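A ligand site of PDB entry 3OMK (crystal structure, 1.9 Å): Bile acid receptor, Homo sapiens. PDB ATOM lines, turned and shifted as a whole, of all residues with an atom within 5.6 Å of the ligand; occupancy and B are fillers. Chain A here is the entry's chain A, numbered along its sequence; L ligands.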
ATOM      1  N   ILE A  30      15.442  34.014  -9.251  1.00  0.00           N
ATOM      2  CA  ILE A  30      15.558  32.567  -9.284  1.00  0.00           C
ATOM      3  C   ILE A  30      15.518  32.076 -10.723  1.00  0.00           C
ATOM      4  O   ILE A  30      16.428  31.363 -11.149  1.00  0.00           O
ATOM      5  CB  ILE A  30      14.409  31.964  -8.413  1.00  0.00           C
ATOM      6  CG1 ILE A  30      14.248  32.807  -7.091  1.00  0.00           C
ATOM      7  CG2 ILE A  30      14.595  30.453  -8.216  1.00  0.00           C
ATOM      8  CD1 ILE A  30      13.385  32.347  -5.950  1.00  0.00           C
ATOM      9  N   THR A  31      14.475  32.461 -11.479  1.00  0.00           N
ATOM     10  CA  THR A  31      14.263  32.050 -12.864  1.00  0.00           C
ATOM     11  C   THR A  31      15.276  32.674 -13.845  1.00  0.00           C
ATOM     12  O   THR A  31      15.524  32.074 -14.888  1.00  0.00           O
ATOM     13  CB  THR A  31      12.801  32.234 -13.289  1.00  0.00           C
ATOM     14  OG1 THR A  31      12.448  33.607 -13.213  1.00  0.00           O
ATOM     15  CG2 THR A  31      11.857  31.433 -12.430  1.00  0.00           C
ATOM     16  N   ILE A  34      18.445  30.324 -13.690  1.00  0.00           N
ATOM     17  CA  ILE A  34      18.166  29.050 -14.354  1.00  0.00           C
ATOM     18  C   ILE A  34      18.060  29.236 -15.874  1.00  0.00           C
ATOM     19  O   ILE A  34      18.557  28.387 -16.604  1.00  0.00           O
ATOM     20  CB  ILE A  34      16.903  28.384 -13.763  1.00  0.00           C
ATOM     21  CG1 ILE A  34      17.042  28.179 -12.228  1.00  0.00           C
ATOM     22  CG2 ILE A  34      16.587  27.049 -14.476  1.00  0.00           C
ATOM     23  CD1 ILE A  34      15.632  27.952 -11.453  1.00  0.00           C
ATOM     24  N   ASN A  44      23.752  22.689  -9.804  1.00  0.00           N
ATOM     25  CA  ASN A  44      22.343  22.852  -9.450  1.00  0.00           C
ATOM     26  C   ASN A  44      22.070  22.444  -8.011  1.00  0.00           C
ATOM     27  O   ASN A  44      21.224  23.077  -7.329  1.00  0.00           O
ATOM     28  CB  ASN A  44      21.437  22.110 -10.438  1.00  0.00           C
ATOM     29  CG  ASN A  44      21.394  22.736 -11.813  1.00  0.00           C
ATOM     30  OD1 ASN A  44      21.248  23.936 -11.963  1.00  0.00           O
ATOM     31  ND2 ASN A  44      21.389  21.921 -12.859  1.00  0.00           N
ATOM     32  N   ILE A  47      22.991  25.338  -5.921  1.00  0.00           N
ATOM     33  CA  ILE A  47      22.029  26.437  -6.108  1.00  0.00           C
ATOM     34  C   ILE A  47      20.808  26.040  -5.251  1.00  0.00           C
ATOM     35  O   ILE A  47      20.297  26.856  -4.509  1.00  0.00           O
ATOM     36  CB  ILE A  47      21.657  26.637  -7.625  1.00  0.00           C
ATOM     37  CG1 ILE A  47      22.830  27.222  -8.438  1.00  0.00           C
ATOM     38  CG2 ILE A  47      20.374  27.448  -7.841  1.00  0.00           C
ATOM     39  CD1 ILE A  47      22.701  27.006  -9.992  1.00  0.00           C
ATOM     40  N   LEU A  48      20.378  24.765  -5.321  1.00  0.00           N
ATOM     41  CA  LEU A  48      19.242  24.317  -4.523  1.00  0.00           C
ATOM     42  C   LEU A  48      19.446  24.468  -3.028  1.00  0.00           C
ATOM     43  O   LEU A  48      18.520  24.909  -2.331  1.00  0.00           O
ATOM     44  CB  LEU A  48      18.866  22.861  -4.843  1.00  0.00           C
ATOM     45  CG  LEU A  48      17.764  22.193  -3.977  1.00  0.00           C
ATOM     46  CD1 LEU A  48      16.392  22.842  -4.149  1.00  0.00           C
ATOM     47  CD2 LEU A  48      17.716  20.714  -4.254  1.00  0.00           C
ATOM     48  N   MET A  51      19.482  28.194  -2.018  1.00  0.00           N
ATOM     49  CA  MET A  51      18.119  28.765  -2.106  1.00  0.00           C
ATOM     50  C   MET A  51      17.266  28.291  -0.951  1.00  0.00           C
ATOM     51  O   MET A  51      16.395  29.026  -0.494  1.00  0.00           O
ATOM     52  CB  MET A  51      17.413  28.316  -3.388  1.00  0.00           C
ATOM     53  CG  MET A  51      17.924  28.953  -4.649  1.00  0.00           C
ATOM     54  SD  MET A  51      17.381  30.640  -4.776  1.00  0.00           S
ATOM     55  CE  MET A  51      15.714  30.414  -4.734  1.00  0.00           C
ATOM     56  N   ALA A  52      17.427  27.018  -0.548  1.00  0.00           N
ATOM     57  CA  ALA A  52      16.637  26.415   0.500  1.00  0.00           C
ATOM     58  C   ALA A  52      17.018  26.893   1.845  1.00  0.00           C
ATOM     59  O   ALA A  52      16.145  26.899   2.695  1.00  0.00           O
ATOM     60  CB  ALA A  52      16.706  24.923   0.440  1.00  0.00           C
ATOM     61  N   HIS A  55      15.455  30.418   2.126  1.00  0.00           N
ATOM     62  CA  HIS A  55      14.035  30.153   2.265  1.00  0.00           C
ATOM     63  C   HIS A  55      13.637  29.722   3.648  1.00  0.00           C
ATOM     64  O   HIS A  55      12.632  30.219   4.160  1.00  0.00           O
ATOM     65  CB  HIS A  55      13.583  29.097   1.237  1.00  0.00           C
ATOM     66  CG  HIS A  55      12.112  28.825   1.270  1.00  0.00           C
ATOM     67  ND1 HIS A  55      11.600  27.754   1.978  1.00  0.00           N
ATOM     68  CD2 HIS A  55      11.091  29.566   0.797  1.00  0.00           C
ATOM     69  CE1 HIS A  55      10.291  27.887   1.943  1.00  0.00           C
ATOM     70  NE2 HIS A  55       9.929  28.951   1.232  1.00  0.00           N
ATOM     71  N   MET A  89       8.428  25.139   0.882  1.00  0.00           N
ATOM     72  CA  MET A  89       9.372  25.307  -0.219  1.00  0.00           C
ATOM     73  C   MET A  89       8.790  24.894  -1.562  1.00  0.00           C
ATOM     74  O   MET A  89       9.014  25.592  -2.572  1.00  0.00           O
ATOM     75  CB  MET A  89      10.652  24.528   0.094  1.00  0.00           C
ATOM     76  CG  MET A  89      11.780  24.835  -0.853  1.00  0.00           C
ATOM     77  SD  MET A  89      11.961  23.424  -1.938  1.00  0.00           S
ATOM     78  CE  MET A  89      13.269  22.659  -1.198  1.00  0.00           C
ATOM     79  N   PHE A  90       8.065  23.755  -1.601  1.00  0.00           N
ATOM     80  CA  PHE A  90       7.497  23.297  -2.866  1.00  0.00           C
ATOM     81  C   PHE A  90       6.326  24.158  -3.281  1.00  0.00           C
ATOM     82  O   PHE A  90       6.048  24.292  -4.467  1.00  0.00           O
ATOM     83  CB  PHE A  90       7.108  21.805  -2.775  1.00  0.00           C
ATOM     84  CG  PHE A  90       8.287  20.843  -2.875  1.00  0.00           C
ATOM     85  CD1 PHE A  90       8.858  20.545  -4.098  1.00  0.00           C
ATOM     86  CD2 PHE A  90       8.738  20.151  -1.764  1.00  0.00           C
ATOM     87  CE1 PHE A  90       9.904  19.655  -4.198  1.00  0.00           C
ATOM     88  CE2 PHE A  90       9.805  19.244  -1.868  1.00  0.00           C
ATOM     89  CZ  PHE A  90      10.364  18.999  -3.086  1.00  0.00           C
ATOM     90  N   ARG A  92       6.166  27.439  -2.762  1.00  0.00           N
ATOM     91  CA  ARG A  92       6.869  28.593  -3.292  1.00  0.00           C
ATOM     92  C   ARG A  92       7.495  28.267  -4.643  1.00  0.00           C
ATOM     93  O   ARG A  92       7.457  29.114  -5.547  1.00  0.00           O
ATOM     94  CB  ARG A  92       7.926  29.084  -2.299  1.00  0.00           C
ATOM     95  CG  ARG A  92       8.678  30.316  -2.833  1.00  0.00           C
ATOM     96  CD  ARG A  92       7.795  31.513  -3.150  1.00  0.00           C
ATOM     97  NE  ARG A  92       8.579  32.733  -3.334  1.00  0.00           N
ATOM     98  CZ  ARG A  92       8.067  33.933  -3.532  1.00  0.00           C
ATOM     99  NH1 ARG A  92       6.756  34.096  -3.606  1.00  0.00           N
ATOM    100  NH2 ARG A  92       8.867  34.998  -3.672  1.00  0.00           N
ATOM    101  N   SER A  93       8.018  27.031  -4.807  1.00  0.00           N
ATOM    102  CA  SER A  93       8.562  26.616  -6.093  1.00  0.00           C
ATOM    103  C   SER A  93       7.436  26.567  -7.146  1.00  0.00           C
ATOM    104  O   SER A  93       7.654  26.978  -8.283  1.00  0.00           O
ATOM    105  CB  SER A  93       9.299  25.296  -5.983  1.00  0.00           C
ATOM    106  OG  SER A  93      10.460  25.468  -5.172  1.00  0.00           O
ATOM    107  N   ALA A  94       6.233  26.121  -6.760  1.00  0.00           N
ATOM    108  CA  ALA A  94       5.050  26.109  -7.627  1.00  0.00           C
ATOM    109  C   ALA A  94       4.595  27.525  -7.977  1.00  0.00           C
ATOM    110  O   ALA A  94       4.196  27.771  -9.117  1.00  0.00           O
ATOM    111  CB  ALA A  94       3.902  25.329  -6.954  1.00  0.00           C
ATOM    112  N   ILE A  96       6.560  30.256  -8.148  1.00  0.00           N
ATOM    113  CA  ILE A  96       7.593  30.728  -9.077  1.00  0.00           C
ATOM    114  C   ILE A  96       7.397  30.075 -10.448  1.00  0.00           C
ATOM    115  O   ILE A  96       7.430  30.771 -11.465  1.00  0.00           O
ATOM    116  CB  ILE A  96       9.014  30.476  -8.532  1.00  0.00           C
ATOM    117  CG1 ILE A  96       9.247  31.238  -7.224  1.00  0.00           C
ATOM    118  CG2 ILE A  96      10.099  30.850  -9.565  1.00  0.00           C
ATOM    119  CD1 ILE A  96      10.382  30.676  -6.454  1.00  0.00           C
ATOM    120  N   PHE A  97       7.216  28.743 -10.476  1.00  0.00           N
ATOM    121  CA  PHE A  97       7.059  28.025 -11.749  1.00  0.00           C
ATOM    122  C   PHE A  97       5.917  28.518 -12.618  1.00  0.00           C
ATOM    123  O   PHE A  97       6.037  28.532 -13.837  1.00  0.00           O
ATOM    124  CB  PHE A  97       6.841  26.545 -11.446  1.00  0.00           C
ATOM    125  CG  PHE A  97       6.876  25.669 -12.670  1.00  0.00           C
ATOM    126  CD1 PHE A  97       8.083  25.329 -13.272  1.00  0.00           C
ATOM    127  CD2 PHE A  97       5.704  25.134 -13.192  1.00  0.00           C
ATOM    128  CE1 PHE A  97       8.116  24.498 -14.394  1.00  0.00           C
ATOM    129  CE2 PHE A  97       5.735  24.313 -14.316  1.00  0.00           C
ATOM    130  CZ  PHE A  97       6.942  23.980 -14.898  1.00  0.00           C
ATOM    131  N   ASN A  98       4.810  28.892 -11.999  1.00  0.00           N
ATOM    132  CA  ASN A  98       3.628  29.294 -12.750  1.00  0.00           C
ATOM    133  C   ASN A  98       3.511  30.781 -13.010  1.00  0.00           C
ATOM    134  O   ASN A  98       2.497  31.212 -13.531  1.00  0.00           O
ATOM    135  CB  ASN A  98       2.357  28.729 -12.081  1.00  0.00           C
ATOM    136  CG  ASN A  98       2.274  27.243 -12.222  1.00  0.00           C
ATOM    137  OD1 ASN A  98       2.055  26.711 -13.318  1.00  0.00           O
ATOM    138  ND2 ASN A  98       2.464  26.552 -11.119  1.00  0.00           N
ATOM    139  N   LEU A 109      12.481  26.888 -18.875  1.00  0.00           N
ATOM    140  CA  LEU A 109      12.643  26.781 -17.427  1.00  0.00           C
ATOM    141  C   LEU A 109      12.313  25.365 -17.007  1.00  0.00           C
ATOM    142  O   LEU A 109      13.085  24.759 -16.290  1.00  0.00           O
ATOM    143  CB  LEU A 109      11.768  27.813 -16.681  1.00  0.00           C
ATOM    144  CG  LEU A 109      11.740  27.706 -15.141  1.00  0.00           C
ATOM    145  CD1 LEU A 109      13.009  28.277 -14.528  1.00  0.00           C
ATOM    146  CD2 LEU A 109      10.459  28.333 -14.567  1.00  0.00           C
ATOM    147  N   ARG A 112      15.158  22.879 -18.114  1.00  0.00           N
ATOM    148  CA  ARG A 112      16.321  23.057 -17.258  1.00  0.00           C
ATOM    149  C   ARG A 112      16.099  22.391 -15.904  1.00  0.00           C
ATOM    150  O   ARG A 112      16.990  21.713 -15.428  1.00  0.00           O
ATOM    151  CB  ARG A 112      16.622  24.547 -17.063  1.00  0.00           C
ATOM    152  CG  ARG A 112      17.116  25.232 -18.328  1.00  0.00           C
ATOM    153  CD  ARG A 112      18.627  25.359 -18.372  1.00  0.00           C
ATOM    154  NE  ARG A 112      19.096  25.852 -19.663  1.00  0.00           N
ATOM    155  CZ  ARG A 112      19.186  27.132 -19.995  1.00  0.00           C
ATOM    156  NH1 ARG A 112      18.850  28.071 -19.136  1.00  0.00           N
ATOM    157  NH2 ARG A 112      19.638  27.489 -21.195  1.00  0.00           N
ATOM    158  N   ILE A 113      14.917  22.547 -15.284  1.00  0.00           N
ATOM    159  CA  ILE A 113      14.620  21.923 -13.972  1.00  0.00           C
ATOM    160  C   ILE A 113      14.659  20.416 -14.146  1.00  0.00           C
ATOM    161  O   ILE A 113      15.329  19.728 -13.393  1.00  0.00           O
ATOM    162  CB  ILE A 113      13.271  22.407 -13.376  1.00  0.00           C
ATOM    163  CG1 ILE A 113      13.280  23.888 -13.066  1.00  0.00           C
ATOM    164  CG2 ILE A 113      12.881  21.592 -12.129  1.00  0.00           C
ATOM    165  CD1 ILE A 113      11.974  24.434 -12.862  1.00  0.00           C
ATOM    166  N   SER A 116      18.104  19.107 -14.154  1.00  0.00           N
ATOM    167  CA  SER A 116      18.891  19.694 -13.074  1.00  0.00           C
ATOM    168  C   SER A 116      19.734  18.695 -12.285  1.00  0.00           C
ATOM    169  O   SER A 116      20.661  19.091 -11.585  1.00  0.00           O
ATOM    170  CB  SER A 116      17.973  20.473 -12.139  1.00  0.00           C
ATOM    171  OG  SER A 116      17.113  19.577 -11.466  1.00  0.00           O
ATOM    172  N   ILE A 118      17.910  15.959 -10.668  1.00  0.00           N
ATOM    173  CA  ILE A 118      16.868  15.244  -9.924  1.00  0.00           C
ATOM    174  C   ILE A 118      16.578  13.934 -10.652  1.00  0.00           C
ATOM    175  O   ILE A 118      16.614  13.888 -11.882  1.00  0.00           O
ATOM    176  CB  ILE A 118      15.618  16.124  -9.719  1.00  0.00           C
ATOM    177  CG1 ILE A 118      14.481  15.328  -9.069  1.00  0.00           C
ATOM    178  CG2 ILE A 118      15.157  16.799 -11.028  1.00  0.00           C
ATOM    179  CD1 ILE A 118      13.443  16.141  -8.473  1.00  0.00           C
ATOM    180  N   MET A 126       6.478  15.909  -9.061  1.00  0.00           N
ATOM    181  CA  MET A 126       6.801  17.324  -8.878  1.00  0.00           C
ATOM    182  C   MET A 126       6.088  18.192  -9.897  1.00  0.00           C
ATOM    183  O   MET A 126       5.381  19.136  -9.510  1.00  0.00           O
ATOM    184  CB  MET A 126       8.323  17.565  -8.887  1.00  0.00           C
ATOM    185  CG  MET A 126       8.674  19.020  -8.927  1.00  0.00           C
ATOM    186  SD  MET A 126      10.433  19.302  -8.724  1.00  0.00           S
ATOM    187  CE  MET A 126      10.980  19.004 -10.307  1.00  0.00           C
ATOM    188  N   TYR A 130       3.025  20.989  -9.674  1.00  0.00           N
ATOM    189  CA  TYR A 130       3.184  22.373 -10.171  1.00  0.00           C
ATOM    190  C   TYR A 130       2.112  22.767 -11.190  1.00  0.00           C
ATOM    191  O   TYR A 130       1.673  23.929 -11.210  1.00  0.00           O
ATOM    192  CB  TYR A 130       4.576  22.579 -10.801  1.00  0.00           C
ATOM    193  CG  TYR A 130       5.761  22.488  -9.884  1.00  0.00           C
ATOM    194  CD1 TYR A 130       5.596  22.496  -8.502  1.00  0.00           C
ATOM    195  CD2 TYR A 130       7.063  22.533 -10.372  1.00  0.00           C
ATOM    196  CE1 TYR A 130       6.694  22.434  -7.651  1.00  0.00           C
ATOM    197  CE2 TYR A 130       8.167  22.480  -9.530  1.00  0.00           C
ATOM    198  CZ  TYR A 130       7.978  22.434  -8.156  1.00  0.00           C
ATOM    199  OH  TYR A 130       9.051  22.325  -7.294  1.00  0.00           O
ATOM    200  N   MET A 211      14.528  12.059  -2.538  1.00  0.00           N
ATOM    201  CA  MET A 211      14.579  12.964  -3.695  1.00  0.00           C
ATOM    202  C   MET A 211      15.925  13.707  -3.660  1.00  0.00           C
ATOM    203  O   MET A 211      16.580  13.820  -4.687  1.00  0.00           O
ATOM    204  CB  MET A 211      13.422  13.969  -3.554  1.00  0.00           C
ATOM    205  CG  MET A 211      13.100  14.764  -4.787  1.00  0.00           C
ATOM    206  SD  MET A 211      11.488  15.528  -4.462  1.00  0.00           S
ATOM    207  CE  MET A 211      11.314  16.614  -5.860  1.00  0.00           C
ATOM    208  N   LEU A 212      16.331  14.186  -2.491  1.00  0.00           N
ATOM    209  CA  LEU A 212      17.601  14.902  -2.313  1.00  0.00           C
ATOM    210  C   LEU A 212      18.839  13.974  -2.426  1.00  0.00           C
ATOM    211  O   LEU A 212      19.829  14.368  -3.042  1.00  0.00           O
ATOM    212  CB  LEU A 212      17.613  15.571  -0.936  1.00  0.00           C
ATOM    213  CG  LEU A 212      16.605  16.689  -0.684  1.00  0.00           C
ATOM    214  CD1 LEU A 212      16.595  17.008   0.806  1.00  0.00           C
ATOM    215  CD2 LEU A 212      16.909  17.922  -1.546  1.00  0.00           C
ATOM    216  N   TRP A 215      19.882  12.779  -6.011  1.00  0.00           N
ATOM    217  CA  TRP A 215      20.313  13.792  -6.944  1.00  0.00           C
ATOM    218  C   TRP A 215      21.557  13.228  -7.592  1.00  0.00           C
ATOM    219  O   TRP A 215      22.422  12.688  -6.885  1.00  0.00           O
ATOM    220  CB  TRP A 215      20.660  15.088  -6.241  1.00  0.00           C
ATOM    221  CG  TRP A 215      20.584  16.253  -7.147  1.00  0.00           C
ATOM    222  CD1 TRP A 215      21.497  16.649  -8.072  1.00  0.00           C
ATOM    223  CD2 TRP A 215      19.476  17.158  -7.269  1.00  0.00           C
ATOM    224  NE1 TRP A 215      21.050  17.764  -8.724  1.00  0.00           N
ATOM    225  CE2 TRP A 215      19.815  18.095  -8.251  1.00  0.00           C
ATOM    226  CE3 TRP A 215      18.229  17.247  -6.630  1.00  0.00           C
ATOM    227  CZ2 TRP A 215      18.970  19.161  -8.598  1.00  0.00           C
ATOM    228  CZ3 TRP A 215      17.372  18.278  -7.003  1.00  0.00           C
ATOM    229  CH2 TRP A 215      17.763  19.242  -7.951  1.00  0.00           C
HETATM  230  N1  LIG L   1      13.234  24.457  -7.806  1.00  0.00           N
HETATM  231  C1  LIG L   1      12.381  23.331  -7.706  1.00  0.00           C
HETATM  232  N2  LIG L   1      11.222  23.507  -8.368  1.00  0.00           N
HETATM  233  C2  LIG L   1      12.566  25.346  -8.647  1.00  0.00           C
HETATM  234  C3  LIG L   1      11.309  24.741  -8.987  1.00  0.00           C
HETATM  235  C4  LIG L   1      14.554  25.865  -6.283  1.00  0.00           C
HETATM  236  C5  LIG L   1      14.548  24.597  -7.213  1.00  0.00           C
HETATM  237  C6  LIG L   1      12.917  26.592  -9.130  1.00  0.00           C
HETATM  238  N3  LIG L   1      13.396  26.112  -5.610  1.00  0.00           N
HETATM  239  C7  LIG L   1      10.400  25.398  -9.854  1.00  0.00           C
HETATM  240  C8  LIG L   1      12.003  27.255  -9.946  1.00  0.00           C
HETATM  241  C9  LIG L   1      12.721  22.198  -6.861  1.00  0.00           C
HETATM  242  C10 LIG L   1      10.762  26.681 -10.274  1.00  0.00           C
HETATM  243  C11 LIG L   1      13.163  27.104  -4.648  1.00  0.00           C
HETATM  244  O1  LIG L   1      15.542  26.589  -6.168  1.00  0.00           O
HETATM  245  C12 LIG L   1      13.723  26.933  -3.361  1.00  0.00           C
HETATM  246  C13 LIG L   1      15.655  24.679  -8.285  1.00  0.00           C
HETATM  247  C14 LIG L   1      12.686  22.375  -5.473  1.00  0.00           C
HETATM  248  C15 LIG L   1      13.177  21.007  -7.410  1.00  0.00           C
HETATM  249  F1  LIG L   1      12.282  28.490 -10.435  1.00  0.00           F
HETATM  250  F2  LIG L   1      10.012  27.414 -11.117  1.00  0.00           F
HETATM  251  C16 LIG L   1      13.534  20.135  -5.197  1.00  0.00           C
HETATM  252  C17 LIG L   1      13.608  19.972  -6.576  1.00  0.00           C
HETATM  253  C18 LIG L   1      13.099  21.339  -4.630  1.00  0.00           C
HETATM  254 CL1  LIG L   1      14.055  18.854  -4.202  1.00  0.00          CL
HETATM  255  C19 LIG L   1      12.397  28.263  -4.948  1.00  0.00           C
HETATM  256  C20 LIG L   1      14.488  25.718  -3.032  1.00  0.00           C
HETATM  257  C21 LIG L   1      13.437  27.858  -2.361  1.00  0.00           C
HETATM  258  C22 LIG L   1      17.054  24.508  -7.707  1.00  0.00           C
HETATM  259  C23 LIG L   1      15.415  23.678  -9.420  1.00  0.00           C
HETATM  260  C24 LIG L   1      12.165  29.198  -3.933  1.00  0.00           C
HETATM  261  C25 LIG L   1      12.693  28.999  -2.664  1.00  0.00           C
HETATM  262  C26 LIG L   1      16.497  23.728 -10.500  1.00  0.00           C
HETATM  263  C27 LIG L   1      18.131  24.518  -8.802  1.00  0.00           C
HETATM  264  C28 LIG L   1      17.849  23.485  -9.873  1.00  0.00           C
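N of Phe 97 sits close to F2 of the ligand, 3.2 Å away. Merely in contact with the ligand: Ile 96 (3.3 Å), Met 126 (3.5 Å), Ile 113 (3.5 Å), Ile 34 (3.5 Å), Thr 31 (3.6 Å), Met 89 (3.6 Å), Leu 109 (3.6 Å), Leu 48 (3.6 Å), Phe 90 (3.6 Å), Met 51 (3.7 Å), Asn 44 (3.7 Å), Ile 30 (3.8 Å), Ser 116 (3.8 Å), His 55 (3.8 Å), Ile 47 (3.8 Å), Arg 92 (3.8 Å) and Met 211 (3.9 Å). 20 residues have an atom within 4 Å of the ligand: Ile 30, Thr 31, Ile 34, Asn 44, Ile 47, Leu 48, Met 51, His 55, Met 89, Phe 90, Arg 92, Ser 93, Ile 96, Phe 97, Leu 109, Ile 113, Ser 116, Met 126, Tyr 130 and Met 211. The nearest printed residue that does not touch the ligand is Leu 212 (4.01 Å).
OH of Tyr 130 lies within hydrogen-bond range of SD of Met 126, at 3.6 Å. The side-chain hydroxyl of Ser 116 lies within hydrogen-bond range of the backbone carbonyl oxygen of Ile 113, 2.6 Å away. The guanidinium group (NH1) of Arg 112 sits at hydrogen-bond distance from the backbone carbonyl oxygen (O) of Ile 34. The backbone carbonyl oxygen (O) of Met 89 is in hydrogen-bond range of the side-chain hydroxyl (OG) of Ser 93. ND2 of Asn 98 sits at hydrogen-bond distance from O of Tyr 130, at 2.7 Å. O of Ser 116 lies within hydrogen-bond range of NE1 of Trp 215 (3.2 Å). ND2 of Asn 44 sits at hydrogen-bond distance from O of Ser 116 (3.2 Å).
The side-chain hydroxyl (OG) of Ser 93 is in hydrogen-bond range of a nitrogen (N3) of the ligand, 3.0 Å away. OH of Tyr 130 lies within hydrogen-bond range of N2 of the ligand (2.7 Å).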
